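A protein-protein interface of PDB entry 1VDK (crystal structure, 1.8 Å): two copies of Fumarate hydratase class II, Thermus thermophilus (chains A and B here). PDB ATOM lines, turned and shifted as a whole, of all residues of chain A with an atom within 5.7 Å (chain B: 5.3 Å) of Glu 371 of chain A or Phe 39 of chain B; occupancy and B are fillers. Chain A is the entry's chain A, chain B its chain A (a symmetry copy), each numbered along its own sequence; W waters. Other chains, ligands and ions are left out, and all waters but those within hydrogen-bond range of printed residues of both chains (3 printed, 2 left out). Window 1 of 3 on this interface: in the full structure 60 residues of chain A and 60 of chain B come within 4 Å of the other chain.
Arg 38 of chain B touches its own counterpart, Arg 38 of chain A. Arg 38 of chain A touches Phe 39 of chain B, and with the chains exchanged Phe 39 of chain A touches Arg 38 of chain B. Arg 38 of chain A touches Tyr 367 of chain B, and with the chains exchanged Tyr 367 of chain A touches Arg 38 of chain B. Phe 39 of chain A touches Glu 371 of chain B, and with the chains exchanged Glu 371 of chain A touches Phe 39 of chain B. 4 positions are printed for both chains.
Of chain B, only Phe 39 (3.4 Å) comes within 4 Å of Glu 371 of chain A. Of the printed residues of chain A, Phe 39 of chain B touches Arg 38 and Glu 371. Of the printed residues of chain B, Leu 375 of chain A touches Gly 35 (3.7 Å) and Phe 95 (3.9 Å). Of the printed residues of chain B, Tyr 367 of chain A touches Arg 38. Printed residues of chain A within 4 Å of Arg 40 of chain B: Arg 38. Printed residues of chain A within 4 Å of Gly 35 of chain B: Leu 375 (3.7 Å). Printed residues of chain A within 4 Å of Arg 38 of chain B: Arg 38, Phe 39 and Tyr 367. Thr 369 of chain A touches none of the printed residues of chain B. The nearest residue of chain B that does not touch Glu 371 of chain A is Glu 371 of chain B (5.1 Å).
The backbone carbonyl oxygen of Arg 38 of chain A sits at hydrogen-bond distance from the guanidinium group of Arg 38 of chain B, at 2.7 Å. The guanidinium group (NH1) of Arg 38 of chain A sits at hydrogen-bond distance from the backbone carbonyl oxygen (O) of Arg 40 of chain B, 2.9 Å away.
The guanidinium group of Arg 339 of chain A lies within salt-bridge range of the side-chain carboxylate of Glu 371 of chain A. The side-chain carboxylate (OE1) of Glu 371 of chain A sits at hydrogen-bond distance from the side-chain amide nitrogen (ND2) of Asn 343 of chain A (2.8 Å). OE2 of Glu 371 of chain A is in hydrogen-bond range of OH of Tyr 367 of chain A, at 2.6 Å. O of Phe 39 of chain B sits at hydrogen-bond distance from N of Val 94 of chain B (2.8 Å). OH of Tyr 367 of chain B lies within hydrogen-bond range of OE2 of Glu 371 of chain B, 2.6 Å away.
Hydrophobic or aromatic side chains of chain A that line the printed part of chain B: Phe 39, Tyr 367 and Leu 375.
Water W3 lies within hydrogen-bond range of O of Met 41 of chain B and NH2 of Arg 38 of chain A. Water W1 bridges ND2 of Asn 374 of chain A (3.2 Å) and NE of Arg 38 of chain B (3.3 Å). Water W2 lies within hydrogen-bond range of O of Arg 38 of chain A (3.2 Å), NH1 of Arg 38 of chain B (3.3 Å) and N of Phe 39 of chain A (3.4 Å).
Among the printed residues, pairs that only touch across the chains: Phe 39 of chain A with Glu 371 of chain B (3.4 Å), Glu 371 of chain A with Phe 39 of chain B (3.4 Å), Arg 38 of chain A with Tyr 367 of chain B (3.5 Å), Tyr 367 of chain A with Arg 38 of chain B (3.5 Å), Arg 38 of chain A with Phe 39 of chain B (3.6 Å), Phe 39 of chain A with Arg 38 of chain B (3.6 Å), Leu 375 of chain A with Gly 35 of chain B (3.7 Å) and Leu 375 of chain A with Phe 95 of chain B (3.9 Å).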
ATOM      1  N   ARG A  38     -31.218  16.479   5.506  1.00  0.00           N
ATOM      2  CA  ARG A  38     -31.058  17.925   5.599  1.00  0.00           C
ATOM      3  C   ARG A  38     -30.371  18.612   4.436  1.00  0.00           C
ATOM      4  O   ARG A  38     -30.392  19.844   4.357  1.00  0.00           O
ATOM      5  CB  ARG A  38     -30.271  18.278   6.861  1.00  0.00           C
ATOM      6  CG  ARG A  38     -30.831  17.716   8.162  1.00  0.00           C
ATOM      7  CD  ARG A  38     -29.863  18.038   9.297  1.00  0.00           C
ATOM      8  NE  ARG A  38     -30.240  17.400  10.557  1.00  0.00           N
ATOM      9  CZ  ARG A  38     -31.170  17.865  11.386  1.00  0.00           C
ATOM     10  NH1 ARG A  38     -31.829  18.984  11.098  1.00  0.00           N
ATOM     11  NH2 ARG A  38     -31.435  17.212  12.512  1.00  0.00           N
ATOM     12  N   PHE A  39     -29.757  17.848   3.542  1.00  0.00           N
ATOM     13  CA  PHE A  39     -29.036  18.476   2.445  1.00  0.00           C
ATOM     14  C   PHE A  39     -29.526  18.252   1.021  1.00  0.00           C
ATOM     15  O   PHE A  39     -28.728  18.069   0.101  1.00  0.00           O
ATOM     16  CB  PHE A  39     -27.550  18.125   2.550  1.00  0.00           C
ATOM     17  CG  PHE A  39     -26.929  18.586   3.838  1.00  0.00           C
ATOM     18  CD1 PHE A  39     -27.005  17.799   4.984  1.00  0.00           C
ATOM     19  CD2 PHE A  39     -26.343  19.845   3.928  1.00  0.00           C
ATOM     20  CE1 PHE A  39     -26.513  18.260   6.204  1.00  0.00           C
ATOM     21  CE2 PHE A  39     -25.848  20.317   5.144  1.00  0.00           C
ATOM     22  CZ  PHE A  39     -25.935  19.518   6.285  1.00  0.00           C
ATOM     23  N   ARG A 339     -22.805  29.861  13.110  1.00  0.00           N
ATOM     24  CA  ARG A 339     -23.015  28.895  12.033  1.00  0.00           C
ATOM     25  C   ARG A 339     -22.494  29.522  10.734  1.00  0.00           C
ATOM     26  O   ARG A 339     -21.809  28.873   9.939  1.00  0.00           O
ATOM     27  CB  ARG A 339     -24.510  28.586  11.879  1.00  0.00           C
ATOM     28  CG  ARG A 339     -24.859  27.606  10.749  1.00  0.00           C
ATOM     29  CD  ARG A 339     -24.466  26.168  11.102  1.00  0.00           C
ATOM     30  NE  ARG A 339     -23.018  25.967  11.067  1.00  0.00           N
ATOM     31  CZ  ARG A 339     -22.317  25.773   9.952  1.00  0.00           C
ATOM     32  NH1 ARG A 339     -22.935  25.741   8.778  1.00  0.00           N
ATOM     33  NH2 ARG A 339     -20.997  25.628  10.004  1.00  0.00           N
ATOM     34  N   ASN A 343     -19.856  28.502   7.796  1.00  0.00           N
ATOM     35  CA  ASN A 343     -20.201  28.406   6.381  1.00  0.00           C
ATOM     36  C   ASN A 343     -19.145  29.116   5.547  1.00  0.00           C
ATOM     37  O   ASN A 343     -18.745  28.632   4.487  1.00  0.00           O
ATOM     38  CB  ASN A 343     -21.583  29.015   6.114  1.00  0.00           C
ATOM     39  CG  ASN A 343     -22.704  28.115   6.582  1.00  0.00           C
ATOM     40  OD1 ASN A 343     -22.555  26.896   6.584  1.00  0.00           O
ATOM     41  ND2 ASN A 343     -23.838  28.702   6.959  1.00  0.00           N
ATOM     42  N   ALA A 366     -22.055  26.565  -3.072  1.00  0.00           N
ATOM     43  CA  ALA A 366     -23.348  27.213  -3.272  1.00  0.00           C
ATOM     44  C   ALA A 366     -24.263  26.963  -2.081  1.00  0.00           C
ATOM     45  O   ALA A 366     -24.934  27.876  -1.598  1.00  0.00           O
ATOM     46  CB  ALA A 366     -24.004  26.694  -4.545  1.00  0.00           C
ATOM     47  N   TYR A 367     -24.280  25.726  -1.599  1.00  0.00           N
ATOM     48  CA  TYR A 367     -25.138  25.379  -0.472  1.00  0.00           C
ATOM     49  C   TYR A 367     -24.837  26.177   0.797  1.00  0.00           C
ATOM     50  O   TYR A 367     -25.744  26.734   1.421  1.00  0.00           O
ATOM     51  CB  TYR A 367     -25.038  23.884  -0.130  1.00  0.00           C
ATOM     52  CG  TYR A 367     -25.768  23.606   1.161  1.00  0.00           C
ATOM     53  CD1 TYR A 367     -27.161  23.583   1.196  1.00  0.00           C
ATOM     54  CD2 TYR A 367     -25.079  23.572   2.374  1.00  0.00           C
ATOM     55  CE1 TYR A 367     -27.852  23.553   2.411  1.00  0.00           C
ATOM     56  CE2 TYR A 367     -25.754  23.545   3.589  1.00  0.00           C
ATOM     57  CZ  TYR A 367     -27.139  23.544   3.602  1.00  0.00           C
ATOM     58  OH  TYR A 367     -27.809  23.597   4.802  1.00  0.00           O
ATOM     59  N   SER A 368     -23.569  26.222   1.195  1.00  0.00           N
ATOM     60  CA  SER A 368     -23.208  26.936   2.411  1.00  0.00           C
ATOM     61  C   SER A 368     -23.460  28.431   2.309  1.00  0.00           C
ATOM     62  O   SER A 368     -23.738  29.084   3.314  1.00  0.00           O
ATOM     63  CB  SER A 368     -21.751  26.660   2.786  1.00  0.00           C
ATOM     64  OG  SER A 368     -21.628  25.333   3.278  1.00  0.00           O
ATOM     65  N   THR A 369     -23.372  28.980   1.103  1.00  0.00           N
ATOM     66  CA  THR A 369     -23.642  30.404   0.955  1.00  0.00           C
ATOM     67  C   THR A 369     -25.154  30.642   1.075  1.00  0.00           C
ATOM     68  O   THR A 369     -25.595  31.569   1.759  1.00  0.00           O
ATOM     69  CB  THR A 369     -23.135  30.942  -0.398  1.00  0.00           C
ATOM     70  OG1 THR A 369     -21.729  30.682  -0.523  1.00  0.00           O
ATOM     71  CG2 THR A 369     -23.367  32.454  -0.482  1.00  0.00           C
ATOM     72  N   LEU A 370     -25.951  29.795   0.426  1.00  0.00           N
ATOM     73  CA  LEU A 370     -27.405  29.940   0.494  1.00  0.00           C
ATOM     74  C   LEU A 370     -27.914  29.698   1.911  1.00  0.00           C
ATOM     75  O   LEU A 370     -28.850  30.354   2.361  1.00  0.00           O
ATOM     76  CB  LEU A 370     -28.082  28.968  -0.477  1.00  0.00           C
ATOM     77  CG  LEU A 370     -27.941  29.399  -1.939  1.00  0.00           C
ATOM     78  CD1 LEU A 370     -28.393  28.281  -2.872  1.00  0.00           C
ATOM     79  CD2 LEU A 370     -28.763  30.666  -2.163  1.00  0.00           C
ATOM     80  N   GLU A 371     -27.302  28.750   2.613  1.00  0.00           N
ATOM     81  CA  GLU A 371     -27.713  28.466   3.987  1.00  0.00           C
ATOM     82  C   GLU A 371     -27.506  29.720   4.831  1.00  0.00           C
ATOM     83  O   GLU A 371     -28.351  30.077   5.651  1.00  0.00           O
ATOM     84  CB  GLU A 371     -26.882  27.319   4.580  1.00  0.00           C
ATOM     85  CG  GLU A 371     -27.321  26.917   5.991  1.00  0.00           C
ATOM     86  CD  GLU A 371     -26.294  26.055   6.701  1.00  0.00           C
ATOM     87  OE1 GLU A 371     -25.597  26.578   7.599  1.00  0.00           O
ATOM     88  OE2 GLU A 371     -26.170  24.861   6.356  1.00  0.00           O
ATOM     89  N   SER A 372     -26.371  30.385   4.631  1.00  0.00           N
ATOM     90  CA  SER A 372     -26.067  31.595   5.387  1.00  0.00           C
ATOM     91  C   SER A 372     -27.091  32.688   5.089  1.00  0.00           C
ATOM     92  O   SER A 372     -27.572  33.372   5.997  1.00  0.00           O
ATOM     93  CB  SER A 372     -24.657  32.095   5.049  1.00  0.00           C
ATOM     94  OG  SER A 372     -23.684  31.095   5.329  1.00  0.00           O
ATOM     95  N   ILE A 373     -27.428  32.840   3.812  1.00  0.00           N
ATOM     96  CA  ILE A 373     -28.402  33.843   3.406  1.00  0.00           C
ATOM     97  C   ILE A 373     -29.773  33.579   4.025  1.00  0.00           C
ATOM     98  O   ILE A 373     -30.404  34.485   4.571  1.00  0.00           O
ATOM     99  CB  ILE A 373     -28.521  33.891   1.862  1.00  0.00           C
ATOM    100  CG1 ILE A 373     -27.228  34.474   1.276  1.00  0.00           C
ATOM    101  CG2 ILE A 373     -29.738  34.729   1.445  1.00  0.00           C
ATOM    102  CD1 ILE A 373     -27.106  34.362  -0.246  1.00  0.00           C
ATOM    103  N   ASN A 374     -30.226  32.334   3.951  1.00  0.00           N
ATOM    104  CA  ASN A 374     -31.530  31.979   4.490  1.00  0.00           C
ATOM    105  C   ASN A 374     -31.620  32.042   6.011  1.00  0.00           C
ATOM    106  O   ASN A 374     -32.612  32.529   6.549  1.00  0.00           O
ATOM    107  CB  ASN A 374     -31.949  30.590   3.992  1.00  0.00           C
ATOM    108  CG  ASN A 374     -32.385  30.603   2.539  1.00  0.00           C
ATOM    109  OD1 ASN A 374     -33.044  31.544   2.094  1.00  0.00           O
ATOM    110  ND2 ASN A 374     -32.036  29.557   1.797  1.00  0.00           N
ATOM    111  N   LEU A 375     -30.594  31.557   6.709  1.00  0.00           N
ATOM    112  CA  LEU A 375     -30.616  31.589   8.170  1.00  0.00           C
ATOM    113  C   LEU A 375     -30.542  33.022   8.684  1.00  0.00           C
ATOM    114  O   LEU A 375     -31.238  33.383   9.630  1.00  0.00           O
ATOM    115  CB  LEU A 375     -29.451  30.780   8.757  1.00  0.00           C
ATOM    116  CG  LEU A 375     -29.559  29.257   8.635  1.00  0.00           C
ATOM    117  CD1 LEU A 375     -28.317  28.591   9.244  1.00  0.00           C
ATOM    118  CD2 LEU A 375     -30.822  28.783   9.351  1.00  0.00           C
ATOM    119  N   LEU A 376     -29.691  33.834   8.066  1.00  0.00           N
ATOM    120  CA  LEU A 376     -29.571  35.227   8.484  1.00  0.00           C
ATOM    121  C   LEU A 376     -30.870  35.975   8.201  1.00  0.00           C
ATOM    122  O   LEU A 376     -31.331  36.762   9.027  1.00  0.00           O
ATOM    123  CB  LEU A 376     -28.403  35.906   7.766  1.00  0.00           C
ATOM    124  CG  LEU A 376     -27.017  35.599   8.345  1.00  0.00           C
ATOM    125  CD1 LEU A 376     -25.948  36.174   7.422  1.00  0.00           C
ATOM    126  CD2 LEU A 376     -26.886  36.195   9.752  1.00  0.00           C
ATOM    127  N   ILE B  34     -36.649  29.807  12.300  1.00  0.00           N
ATOM    128  CA  ILE B  34     -35.293  29.961  11.794  1.00  0.00           C
ATOM    129  C   ILE B  34     -34.748  28.593  11.425  1.00  0.00           C
ATOM    130  O   ILE B  34     -34.511  27.758  12.303  1.00  0.00           O
ATOM    131  CB  ILE B  34     -34.407  30.618  12.879  1.00  0.00           C
ATOM    132  CG1 ILE B  34     -35.024  31.965  13.281  1.00  0.00           C
ATOM    133  CG2 ILE B  34     -32.981  30.803  12.368  1.00  0.00           C
ATOM    134  CD1 ILE B  34     -34.420  32.586  14.534  1.00  0.00           C
ATOM    135  N   GLY B  35     -34.573  28.371  10.124  1.00  0.00           N
ATOM    136  CA  GLY B  35     -34.070  27.094   9.631  1.00  0.00           C
ATOM    137  C   GLY B  35     -35.056  25.955   9.835  1.00  0.00           C
ATOM    138  O   GLY B  35     -34.663  24.822  10.115  1.00  0.00           O
ATOM    139  N   THR B  36     -36.344  26.238   9.677  1.00  0.00           N
ATOM    140  CA  THR B  36     -37.361  25.214   9.892  1.00  0.00           C
ATOM    141  C   THR B  36     -37.265  24.001   8.968  1.00  0.00           C
ATOM    142  O   THR B  36     -37.590  22.882   9.373  1.00  0.00           O
ATOM    143  CB  THR B  36     -38.780  25.820   9.791  1.00  0.00           C
ATOM    144  OG1 THR B  36     -38.998  26.320   8.471  1.00  0.00           O
ATOM    145  CG2 THR B  36     -38.932  26.969  10.776  1.00  0.00           C
ATOM    146  N   ASP B  37     -36.805  24.207   7.737  1.00  0.00           N
ATOM    147  CA  ASP B  37     -36.703  23.101   6.790  1.00  0.00           C
ATOM    148  C   ASP B  37     -35.544  22.136   7.023  1.00  0.00           C
ATOM    149  O   ASP B  37     -35.730  20.919   7.001  1.00  0.00           O
ATOM    150  CB  ASP B  37     -36.621  23.636   5.353  1.00  0.00           C
ATOM    151  CG  ASP B  37     -37.912  24.287   4.898  1.00  0.00           C
ATOM    152  OD1 ASP B  37     -38.957  23.604   4.907  1.00  0.00           O
ATOM    153  OD2 ASP B  37     -37.884  25.481   4.531  1.00  0.00           O
ATOM    154  N   ARG B  38     -34.354  22.672   7.262  1.00  0.00           N
ATOM    155  CA  ARG B  38     -33.176  21.829   7.430  1.00  0.00           C
ATOM    156  C   ARG B  38     -32.623  21.701   8.836  1.00  0.00           C
ATOM    157  O   ARG B  38     -31.766  20.846   9.077  1.00  0.00           O
ATOM    158  CB  ARG B  38     -32.041  22.342   6.543  1.00  0.00           C
ATOM    159  CG  ARG B  38     -32.383  22.498   5.066  1.00  0.00           C
ATOM    160  CD  ARG B  38     -31.201  23.146   4.352  1.00  0.00           C
ATOM    161  NE  ARG B  38     -31.498  23.479   2.960  1.00  0.00           N
ATOM    162  CZ  ARG B  38     -31.467  22.609   1.955  1.00  0.00           C
ATOM    163  NH1 ARG B  38     -31.148  21.337   2.177  1.00  0.00           N
ATOM    164  NH2 ARG B  38     -31.750  23.015   0.722  1.00  0.00           N
ATOM    165  N   PHE B  39     -33.085  22.534   9.759  1.00  0.00           N
ATOM    166  CA  PHE B  39     -32.532  22.480  11.106  1.00  0.00           C
ATOM    167  C   PHE B  39     -33.443  22.073  12.255  1.00  0.00           C
ATOM    168  O   PHE B  39     -33.378  22.645  13.344  1.00  0.00           O
ATOM    169  CB  PHE B  39     -31.846  23.810  11.424  1.00  0.00           C
ATOM    170  CG  PHE B  39     -30.727  24.134  10.476  1.00  0.00           C
ATOM    171  CD1 PHE B  39     -30.985  24.770   9.265  1.00  0.00           C
ATOM    172  CD2 PHE B  39     -29.426  23.726  10.754  1.00  0.00           C
ATOM    173  CE1 PHE B  39     -29.965  24.991   8.340  1.00  0.00           C
ATOM    174  CE2 PHE B  39     -28.398  23.941   9.836  1.00  0.00           C
ATOM    175  CZ  PHE B  39     -28.673  24.576   8.624  1.00  0.00           C
ATOM    176  N   ARG B  40     -34.289  21.081  12.020  1.00  0.00           N
ATOM    177  CA  ARG B  40     -35.129  20.603  13.101  1.00  0.00           C
ATOM    178  C   ARG B  40     -34.137  19.993  14.091  1.00  0.00           C
ATOM    179  O   ARG B  40     -33.123  19.432  13.680  1.00  0.00           O
ATOM    180  CB  ARG B  40     -36.098  19.529  12.612  1.00  0.00           C
ATOM    181  CG  ARG B  40     -36.898  18.926  13.752  1.00  0.00           C
ATOM    182  CD  ARG B  40     -38.207  18.382  13.282  1.00  0.00           C
ATOM    183  NE  ARG B  40     -39.020  19.403  12.626  1.00  0.00           N
ATOM    184  CZ  ARG B  40     -40.223  19.154  12.123  1.00  0.00           C
ATOM    185  NH1 ARG B  40     -40.725  17.931  12.215  1.00  0.00           N
ATOM    186  NH2 ARG B  40     -40.915  20.113  11.528  1.00  0.00           N
ATOM    187  N   MET B  41     -34.413  20.123  15.382  1.00  0.00           N
ATOM    188  CA  MET B  41     -33.524  19.578  16.409  1.00  0.00           C
ATOM    189  C   MET B  41     -33.224  18.106  16.101  1.00  0.00           C
ATOM    190  O   MET B  41     -34.134  17.328  15.816  1.00  0.00           O
ATOM    191  CB  MET B  41     -34.190  19.706  17.783  1.00  0.00           C
ATOM    192  CG  MET B  41     -33.317  19.321  18.971  1.00  0.00           C
ATOM    193  SD  MET B  41     -31.913  20.430  19.216  1.00  0.00           S
ATOM    194  CE  MET B  41     -32.722  21.908  19.848  1.00  0.00           C
ATOM    195  N   LEU B  92     -39.544  21.564  16.842  1.00  0.00           N
ATOM    196  CA  LEU B  92     -38.704  22.735  17.066  1.00  0.00           C
ATOM    197  C   LEU B  92     -37.349  22.697  16.369  1.00  0.00           C
ATOM    198  O   LEU B  92     -36.809  21.626  16.089  1.00  0.00           O
ATOM    199  CB  LEU B  92     -38.503  22.941  18.568  1.00  0.00           C
ATOM    200  CG  LEU B  92     -39.784  22.882  19.409  1.00  0.00           C
ATOM    201  CD1 LEU B  92     -39.437  23.193  20.859  1.00  0.00           C
ATOM    202  CD2 LEU B  92     -40.813  23.887  18.877  1.00  0.00           C
ATOM    203  N   VAL B  93     -36.807  23.885  16.101  1.00  0.00           N
ATOM    204  CA  VAL B  93     -35.519  24.017  15.422  1.00  0.00           C
ATOM    205  C   VAL B  93     -34.335  24.166  16.370  1.00  0.00           C
ATOM    206  O   VAL B  93     -34.487  24.416  17.567  1.00  0.00           O
ATOM    207  CB  VAL B  93     -35.497  25.251  14.472  1.00  0.00           C
ATOM    208  CG1 VAL B  93     -36.593  25.131  13.428  1.00  0.00           C
ATOM    209  CG2 VAL B  93     -35.647  26.535  15.273  1.00  0.00           C
ATOM    210  N   VAL B  94     -33.143  24.024  15.800  1.00  0.00           N
ATOM    211  CA  VAL B  94     -31.900  24.167  16.533  1.00  0.00           C
ATOM    212  C   VAL B  94     -31.750  25.611  17.006  1.00  0.00           C
ATOM    213  O   VAL B  94     -31.286  25.876  18.120  1.00  0.00           O
ATOM    214  CB  VAL B  94     -30.699  23.814  15.617  1.00  0.00           C
ATOM    215  CG1 VAL B  94     -29.375  24.231  16.278  1.00  0.00           C
ATOM    216  CG2 VAL B  94     -30.711  22.318  15.317  1.00  0.00           C
ATOM    217  N   PHE B  95     -32.168  26.549  16.161  1.00  0.00           N
ATOM    218  CA  PHE B  95     -32.036  27.963  16.474  1.00  0.00           C
ATOM    219  C   PHE B  95     -33.164  28.544  17.326  1.00  0.00           C
ATOM    220  O   PHE B  95     -33.944  29.395  16.884  1.00  0.00           O
ATOM    221  CB  PHE B  95     -31.849  28.737  15.164  1.00  0.00           C
ATOM    222  CG  PHE B  95     -30.662  28.266  14.372  1.00  0.00           C
ATOM    223  CD1 PHE B  95     -30.826  27.447  13.256  1.00  0.00           C
ATOM    224  CD2 PHE B  95     -29.369  28.571  14.796  1.00  0.00           C
ATOM    225  CE1 PHE B  95     -29.722  26.934  12.577  1.00  0.00           C
ATOM    226  CE2 PHE B  95     -28.253  28.060  14.122  1.00  0.00           C
ATOM    227  CZ  PHE B  95     -28.431  27.241  13.012  1.00  0.00           C
ATOM    228  N   TYR B 367     -25.632  20.486  17.425  1.00  0.00           N
ATOM    229  CA  TYR B 367     -26.054  20.256  16.047  1.00  0.00           C
ATOM    230  C   TYR B 367     -24.891  20.118  15.065  1.00  0.00           C
ATOM    231  O   TYR B 367     -24.845  19.173  14.273  1.00  0.00           O
ATOM    232  CB  TYR B 367     -26.971  21.383  15.546  1.00  0.00           C
ATOM    233  CG  TYR B 367     -27.212  21.222  14.066  1.00  0.00           C
ATOM    234  CD1 TYR B 367     -28.070  20.230  13.591  1.00  0.00           C
ATOM    235  CD2 TYR B 367     -26.435  21.918  13.139  1.00  0.00           C
ATOM    236  CE1 TYR B 367     -28.132  19.922  12.230  1.00  0.00           C
ATOM    237  CE2 TYR B 367     -26.485  21.618  11.782  1.00  0.00           C
ATOM    238  CZ  TYR B 367     -27.328  20.615  11.334  1.00  0.00           C
ATOM    239  OH  TYR B 367     -27.321  20.262  10.005  1.00  0.00           O
ATOM    240  N   GLU B 371     -23.957  16.855  12.950  1.00  0.00           N
ATOM    241  CA  GLU B 371     -23.982  16.942  11.491  1.00  0.00           C
ATOM    242  C   GLU B 371     -22.679  16.368  10.942  1.00  0.00           C
ATOM    243  O   GLU B 371     -22.678  15.631   9.956  1.00  0.00           O
ATOM    244  CB  GLU B 371     -24.121  18.401  11.033  1.00  0.00           C
ATOM    245  CG  GLU B 371     -24.237  18.552   9.514  1.00  0.00           C
ATOM    246  CD  GLU B 371     -24.012  19.979   9.048  1.00  0.00           C
ATOM    247  OE1 GLU B 371     -22.924  20.261   8.498  1.00  0.00           O
ATOM    248  OE2 GLU B 371     -24.912  20.823   9.241  1.00  0.00           O
HETATM  249  O   HOH W   1     -31.121  26.780   2.971  1.00  0.00           O
HETATM  250  O   HOH W   2     -33.011  18.642   2.872  1.00  0.00           O
HETATM  251  O   HOH W   3     -34.496  16.094  13.144  1.00  0.00           O
